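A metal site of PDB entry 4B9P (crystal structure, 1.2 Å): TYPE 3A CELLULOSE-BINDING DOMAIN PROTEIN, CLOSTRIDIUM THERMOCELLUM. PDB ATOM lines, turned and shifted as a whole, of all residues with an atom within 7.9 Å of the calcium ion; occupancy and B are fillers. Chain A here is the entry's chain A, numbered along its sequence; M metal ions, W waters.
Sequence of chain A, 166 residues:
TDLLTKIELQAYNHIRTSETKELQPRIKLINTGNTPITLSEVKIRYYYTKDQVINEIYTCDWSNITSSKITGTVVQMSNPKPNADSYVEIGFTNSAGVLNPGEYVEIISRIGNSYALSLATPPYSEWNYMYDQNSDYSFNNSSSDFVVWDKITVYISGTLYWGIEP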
ATOM      1  N   SER A  18      13.482  31.522 -19.063  1.00  0.00           N
ATOM      2  CA  SER A  18      13.764  31.014 -20.407  1.00  0.00           C
ATOM      3  C   SER A  18      15.253  31.138 -20.759  1.00  0.00           C
ATOM      4  O   SER A  18      15.846  30.223 -21.336  1.00  0.00           O
ATOM      5  CB  SER A  18      12.932  31.773 -21.421  1.00  0.00           C
ATOM      6  OG  SER A  18      13.065  33.160 -21.220  1.00  0.00           O
ATOM      7  N   LEU A  23      22.774  26.924 -15.664  1.00  0.00           N
ATOM      8  CA  LEU A  23      21.827  25.829 -15.450  1.00  0.00           C
ATOM      9  C   LEU A  23      21.908  25.422 -14.001  1.00  0.00           C
ATOM     10  O   LEU A  23      22.999  25.265 -13.466  1.00  0.00           O
ATOM     11  CB  LEU A  23      22.194  24.633 -16.325  1.00  0.00           C
ATOM     12  CG  LEU A  23      22.416  24.903 -17.799  1.00  0.00           C
ATOM     13  CD1 LEU A  23      22.790  23.608 -18.550  1.00  0.00           C
ATOM     14  CD2 LEU A  23      21.196  25.560 -18.432  1.00  0.00           C
ATOM     15  N   TYR A  47      20.346  16.334 -20.006  1.00  0.00           N
ATOM     16  CA  TYR A  47      20.538  16.626 -21.432  1.00  0.00           C
ATOM     17  C   TYR A  47      20.062  18.030 -21.783  1.00  0.00           C
ATOM     18  O   TYR A  47      19.008  18.472 -21.303  1.00  0.00           O
ATOM     19  CB  TYR A  47      19.730  15.650 -22.270  1.00  0.00           C
ATOM     20  CG  TYR A  47      20.182  14.238 -22.211  1.00  0.00           C
ATOM     21  CD1 TYR A  47      21.255  13.803 -23.007  1.00  0.00           C
ATOM     22  CD2 TYR A  47      19.581  13.326 -21.340  1.00  0.00           C
ATOM     23  CE1 TYR A  47      21.658  12.470 -22.999  1.00  0.00           C
ATOM     24  CE2 TYR A  47      19.996  12.022 -21.304  1.00  0.00           C
ATOM     25  CZ  TYR A  47      21.029  11.593 -22.107  1.00  0.00           C
ATOM     26  OH  TYR A  47      21.389  10.253 -22.019  1.00  0.00           O
ATOM     27  N   TYR A  48      20.813  18.710 -22.640  1.00  0.00           N
ATOM     28  CA  TYR A  48      20.464  20.097 -22.961  1.00  0.00           C
ATOM     29  C   TYR A  48      21.122  20.450 -24.297  1.00  0.00           C
ATOM     30  O   TYR A  48      21.908  19.667 -24.871  1.00  0.00           O
ATOM     31  CB  TYR A  48      20.938  21.027 -21.836  1.00  0.00           C
ATOM     32  CG  TYR A  48      22.449  21.171 -21.673  1.00  0.00           C
ATOM     33  CD1 TYR A  48      23.209  20.192 -21.005  1.00  0.00           C
ATOM     34  CD2 TYR A  48      23.100  22.307 -22.139  1.00  0.00           C
ATOM     35  CE1 TYR A  48      24.556  20.308 -20.868  1.00  0.00           C
ATOM     36  CE2 TYR A  48      24.482  22.444 -21.951  1.00  0.00           C
ATOM     37  CZ  TYR A  48      25.186  21.446 -21.308  1.00  0.00           C
ATOM     38  OH  TYR A  48      26.535  21.569 -21.150  1.00  0.00           O
ATOM     39  N   THR A  49      20.785  21.635 -24.793  1.00  0.00           N
ATOM     40  CA  THR A  49      21.514  22.221 -25.938  1.00  0.00           C
ATOM     41  C   THR A  49      22.367  23.382 -25.447  1.00  0.00           C
ATOM     42  O   THR A  49      21.868  24.310 -24.806  1.00  0.00           O
ATOM     43  CB  THR A  49      20.528  22.693 -27.002  1.00  0.00           C
ATOM     44  OG1 THR A  49      19.480  23.455 -26.368  1.00  0.00           O
ATOM     45  CG2 THR A  49      19.950  21.482 -27.784  1.00  0.00           C
ATOM     46  N   LYS A  50      23.674  23.295 -25.708  1.00  0.00           N
ATOM     47  CA  LYS A  50      24.633  24.317 -25.212  1.00  0.00           C
ATOM     48  C   LYS A  50      24.465  25.665 -25.884  1.00  0.00           C
ATOM     49  O   LYS A  50      25.002  26.656 -25.392  1.00  0.00           O
ATOM     50  CB  LYS A  50      26.071  23.819 -25.366  1.00  0.00           C
ATOM     51  CG  LYS A  50      26.493  23.708 -26.848  1.00  0.00           C
ATOM     52  CD  LYS A  50      27.898  23.184 -27.005  1.00  0.00           C
ATOM     53  CE  LYS A  50      28.374  23.200 -28.462  1.00  0.00           C
ATOM     54  NZ  LYS A  50      27.560  22.325 -29.322  1.00  0.00           N
ATOM     55  N   ASP A  51      23.723  25.714 -26.991  1.00  0.00           N
ATOM     56  CA  ASP A  51      23.482  26.972 -27.687  1.00  0.00           C
ATOM     57  C   ASP A  51      24.832  27.571 -28.060  1.00  0.00           C
ATOM     58  O   ASP A  51      25.649  26.852 -28.648  1.00  0.00           O
ATOM     59  CB  ASP A  51      22.561  27.859 -26.863  1.00  0.00           C
ATOM     60  CG  ASP A  51      21.327  27.098 -26.323  1.00  0.00           C
ATOM     61  OD1 ASP A  51      20.744  26.251 -27.052  1.00  0.00           O
ATOM     62  OD2 ASP A  51      20.934  27.366 -25.182  1.00  0.00           O
ATOM     63  N   GLN A  52      25.093  28.857 -27.793  1.00  0.00           N
ATOM     64  CA  GLN A  52      26.408  29.429 -28.110  1.00  0.00           C
ATOM     65  C   GLN A  52      27.293  29.627 -26.883  1.00  0.00           C
ATOM     66  O   GLN A  52      28.292  30.339 -26.951  1.00  0.00           O
ATOM     67  CB  GLN A  52      26.214  30.734 -28.889  1.00  0.00           C
ATOM     68  CG  GLN A  52      25.578  30.499 -30.261  1.00  0.00           C
ATOM     69  CD  GLN A  52      25.428  31.769 -31.020  1.00  0.00           C
ATOM     70  OE1 GLN A  52      24.497  32.577 -30.751  1.00  0.00           O
ATOM     71  NE2 GLN A  52      26.351  32.017 -31.930  1.00  0.00           N
ATOM     72  N   VAL A  53      26.950  28.991 -25.769  1.00  0.00           N
ATOM     73  CA  VAL A  53      27.713  29.186 -24.563  1.00  0.00           C
ATOM     74  C   VAL A  53      29.055  28.472 -24.651  1.00  0.00           C
ATOM     75  O   VAL A  53      29.138  27.370 -25.178  1.00  0.00           O
ATOM     76  CB  VAL A  53      26.883  28.681 -23.339  1.00  0.00           C
ATOM     77  CG1 VAL A  53      27.696  28.794 -22.057  1.00  0.00           C
ATOM     78  CG2 VAL A  53      25.590  29.518 -23.239  1.00  0.00           C
ATOM     79  N   ASN A  83      16.883  19.001 -29.039  1.00  0.00           N
ATOM     80  CA  ASN A  83      16.895  19.434 -27.636  1.00  0.00           C
ATOM     81  C   ASN A  83      17.981  18.764 -26.807  1.00  0.00           C
ATOM     82  O   ASN A  83      18.006  18.886 -25.578  1.00  0.00           O
ATOM     83  CB  ASN A  83      15.517  19.285 -26.971  1.00  0.00           C
ATOM     84  CG  ASN A  83      14.473  20.036 -27.727  1.00  0.00           C
ATOM     85  OD1 ASN A  83      14.478  21.242 -27.727  1.00  0.00           O
ATOM     86  ND2 ASN A  83      13.575  19.342 -28.396  1.00  0.00           N
ATOM     87  N   ALA A  84      18.919  18.114 -27.495  1.00  0.00           N
ATOM     88  CA  ALA A  84      20.008  17.480 -26.748  1.00  0.00           C
ATOM     89  C   ALA A  84      21.270  17.373 -27.602  1.00  0.00           C
ATOM     90  O   ALA A  84      21.392  16.460 -28.434  1.00  0.00           O
ATOM     91  CB  ALA A  84      19.602  16.079 -26.242  1.00  0.00           C
ATOM     92  N   ASP A  85      22.197  18.304 -27.422  1.00  0.00           N
ATOM     93  CA  ASP A  85      23.479  18.144 -28.040  1.00  0.00           C
ATOM     94  C   ASP A  85      24.585  18.020 -27.020  1.00  0.00           C
ATOM     95  O   ASP A  85      25.747  17.863 -27.420  1.00  0.00           O
ATOM     96  CB  ASP A  85      23.827  19.203 -29.112  1.00  0.00           C
ATOM     97  CG  ASP A  85      24.254  20.590 -28.540  1.00  0.00           C
ATOM     98  OD1 ASP A  85      24.148  20.813 -27.287  1.00  0.00           O
ATOM     99  OD2 ASP A  85      24.693  21.443 -29.366  1.00  0.00           O
ATOM    100  N   MET A 130      24.734  33.128 -22.193  1.00  0.00           N
ATOM    101  CA  MET A 130      23.311  32.968 -21.905  1.00  0.00           C
ATOM    102  C   MET A 130      22.778  31.717 -22.619  1.00  0.00           C
ATOM    103  O   MET A 130      22.819  31.624 -23.847  1.00  0.00           O
ATOM    104  CB  MET A 130      22.562  34.202 -22.389  1.00  0.00           C
ATOM    105  CG  MET A 130      21.165  34.317 -21.817  1.00  0.00           C
ATOM    106  SD  MET A 130      21.152  34.783 -20.048  1.00  0.00           S
ATOM    107  CE  MET A 130      21.303  36.579 -20.218  1.00  0.00           C
ATOM    108  N   TYR A 131      22.293  30.753 -21.832  1.00  0.00           N
ATOM    109  CA  TYR A 131      21.576  29.589 -22.340  1.00  0.00           C
ATOM    110  C   TYR A 131      20.130  29.891 -22.609  1.00  0.00           C
ATOM    111  O   TYR A 131      19.499  30.683 -21.880  1.00  0.00           O
ATOM    112  CB  TYR A 131      21.568  28.530 -21.281  1.00  0.00           C
ATOM    113  CG  TYR A 131      22.904  27.869 -20.993  1.00  0.00           C
ATOM    114  CD1 TYR A 131      23.502  27.027 -21.920  1.00  0.00           C
ATOM    115  CD2 TYR A 131      23.516  28.040 -19.764  1.00  0.00           C
ATOM    116  CE1 TYR A 131      24.687  26.365 -21.608  1.00  0.00           C
ATOM    117  CE2 TYR A 131      24.671  27.368 -19.434  1.00  0.00           C
ATOM    118  CZ  TYR A 131      25.244  26.513 -20.354  1.00  0.00           C
ATOM    119  OH  TYR A 131      26.413  25.858 -20.027  1.00  0.00           O
ATOM    120  N   ASP A 132      19.540  29.175 -23.591  1.00  0.00           N
ATOM    121  CA  ASP A 132      18.093  29.086 -23.743  1.00  0.00           C
ATOM    122  C   ASP A 132      17.662  27.759 -23.162  1.00  0.00           C
ATOM    123  O   ASP A 132      18.084  26.701 -23.662  1.00  0.00           O
ATOM    124  CB  ASP A 132      17.743  29.159 -25.230  1.00  0.00           C
ATOM    125  CG  ASP A 132      16.297  28.900 -25.470  1.00  0.00           C
ATOM    126  OD1 ASP A 132      15.874  27.728 -25.662  1.00  0.00           O
ATOM    127  OD2 ASP A 132      15.537  29.885 -25.488  1.00  0.00           O
ATOM    128  N   GLN A 133      16.797  27.766 -22.132  1.00  0.00           N
ATOM    129  CA  GLN A 133      16.468  26.509 -21.439  1.00  0.00           C
ATOM    130  C   GLN A 133      15.337  25.734 -22.080  1.00  0.00           C
ATOM    131  O   GLN A 133      15.254  24.536 -21.883  1.00  0.00           O
ATOM    132  CB  GLN A 133      16.135  26.748 -19.967  1.00  0.00           C
ATOM    133  CG  GLN A 133      17.277  27.396 -19.189  1.00  0.00           C
ATOM    134  CD  GLN A 133      17.222  27.131 -17.724  1.00  0.00           C
ATOM    135  OE1 GLN A 133      17.734  26.095 -17.285  1.00  0.00           O
ATOM    136  NE2 GLN A 133      16.549  27.989 -16.958  1.00  0.00           N
ATOM    137  N   ASN A 134      14.421  26.383 -22.770  1.00  0.00           N
ATOM    138  CA  ASN A 134      13.276  25.618 -23.293  1.00  0.00           C
ATOM    139  C   ASN A 134      13.707  24.681 -24.414  1.00  0.00           C
ATOM    140  O   ASN A 134      12.971  23.739 -24.725  1.00  0.00           O
ATOM    141  CB  ASN A 134      12.198  26.582 -23.762  1.00  0.00           C
ATOM    142  CG  ASN A 134      11.528  27.295 -22.625  1.00  0.00           C
ATOM    143  OD1 ASN A 134      11.503  28.515 -22.573  1.00  0.00           O
ATOM    144  ND2 ASN A 134      11.001  26.528 -21.695  1.00  0.00           N
ATOM    145  N   SER A 135      14.905  24.870 -24.945  1.00  0.00           N
ATOM    146  CA  SER A 135      15.518  23.990 -25.943  1.00  0.00           C
ATOM    147  C   SER A 135      16.284  22.828 -25.300  1.00  0.00           C
ATOM    148  O   SER A 135      17.095  22.181 -25.966  1.00  0.00           O
ATOM    149  CB  SER A 135      16.459  24.808 -26.844  1.00  0.00           C
ATOM    150  OG  SER A 135      17.400  25.543 -26.062  1.00  0.00           O
ATOM    151  N   ASP A 136      16.093  22.613 -23.997  1.00  0.00           N
ATOM    152  CA  ASP A 136      16.856  21.590 -23.265  1.00  0.00           C
ATOM    153  C   ASP A 136      15.950  20.443 -22.865  1.00  0.00           C
ATOM    154  O   ASP A 136      15.012  20.631 -22.076  1.00  0.00           O
ATOM    155  CB  ASP A 136      17.508  22.184 -22.003  1.00  0.00           C
ATOM    156  CG  ASP A 136      18.456  23.330 -22.318  1.00  0.00           C
ATOM    157  OD1 ASP A 136      18.860  23.457 -23.494  1.00  0.00           O
ATOM    158  OD2 ASP A 136      18.853  24.008 -21.346  1.00  0.00           O
ATOM    159  N   TYR A 137      16.271  19.248 -23.357  1.00  0.00           N
ATOM    160  CA  TYR A 137      15.448  18.061 -23.116  1.00  0.00           C
ATOM    161  C   TYR A 137      15.120  17.873 -21.658  1.00  0.00           C
ATOM    162  O   TYR A 137      13.980  17.573 -21.322  1.00  0.00           O
ATOM    163  CB  TYR A 137      16.153  16.856 -23.680  1.00  0.00           C
ATOM    164  CG  TYR A 137      15.428  15.543 -23.465  1.00  0.00           C
ATOM    165  CD1 TYR A 137      14.385  15.177 -24.302  1.00  0.00           C
ATOM    166  CD2 TYR A 137      15.815  14.657 -22.470  1.00  0.00           C
ATOM    167  CE1 TYR A 137      13.747  13.962 -24.153  1.00  0.00           C
ATOM    168  CE2 TYR A 137      15.155  13.436 -22.292  1.00  0.00           C
ATOM    169  CZ  TYR A 137      14.145  13.098 -23.152  1.00  0.00           C
ATOM    170  OH  TYR A 137      13.467  11.912 -23.007  1.00  0.00           O
HETATM  171 CA    CA M   1      19.637  25.323 -24.838  1.00  0.00          CA
HETATM  172  O   HOH W   1      20.582  25.668 -22.573  1.00  0.00           O
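Within 4 Å of the calcium ion: Thr 49, Asp 51, Asp 132, Ser 135 and Asp 136.
The backbone carbonyl oxygen (O) of Ser 135 sits close to the side-chain amide oxygen (OD1) of Asn 83 (3.3 Å).
The calcium ion is bound by the backbone carbonyl oxygen (O) of Asp 132 (2.4 Å).
OG1 of Thr 49 is bound to the calcium ion.
The calcium ion is bound by OD1 of Asp 136 (2.4 Å).
OD2 of Asp 51 is bound to the calcium ion (2.4 Å).
O of Thr 49 is bound to the calcium ion, 2.5 Å away.
The calcium ion is bound by water W1 (2.5 Å).
The calcium ion is bound by the side-chain hydroxyl (OG) of Ser 135 (2.6 Å).
OD1 of Asp 51 is bound to the calcium ion, at 2.6 Å.
The calcium ion has eight donor atoms within binding distance.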
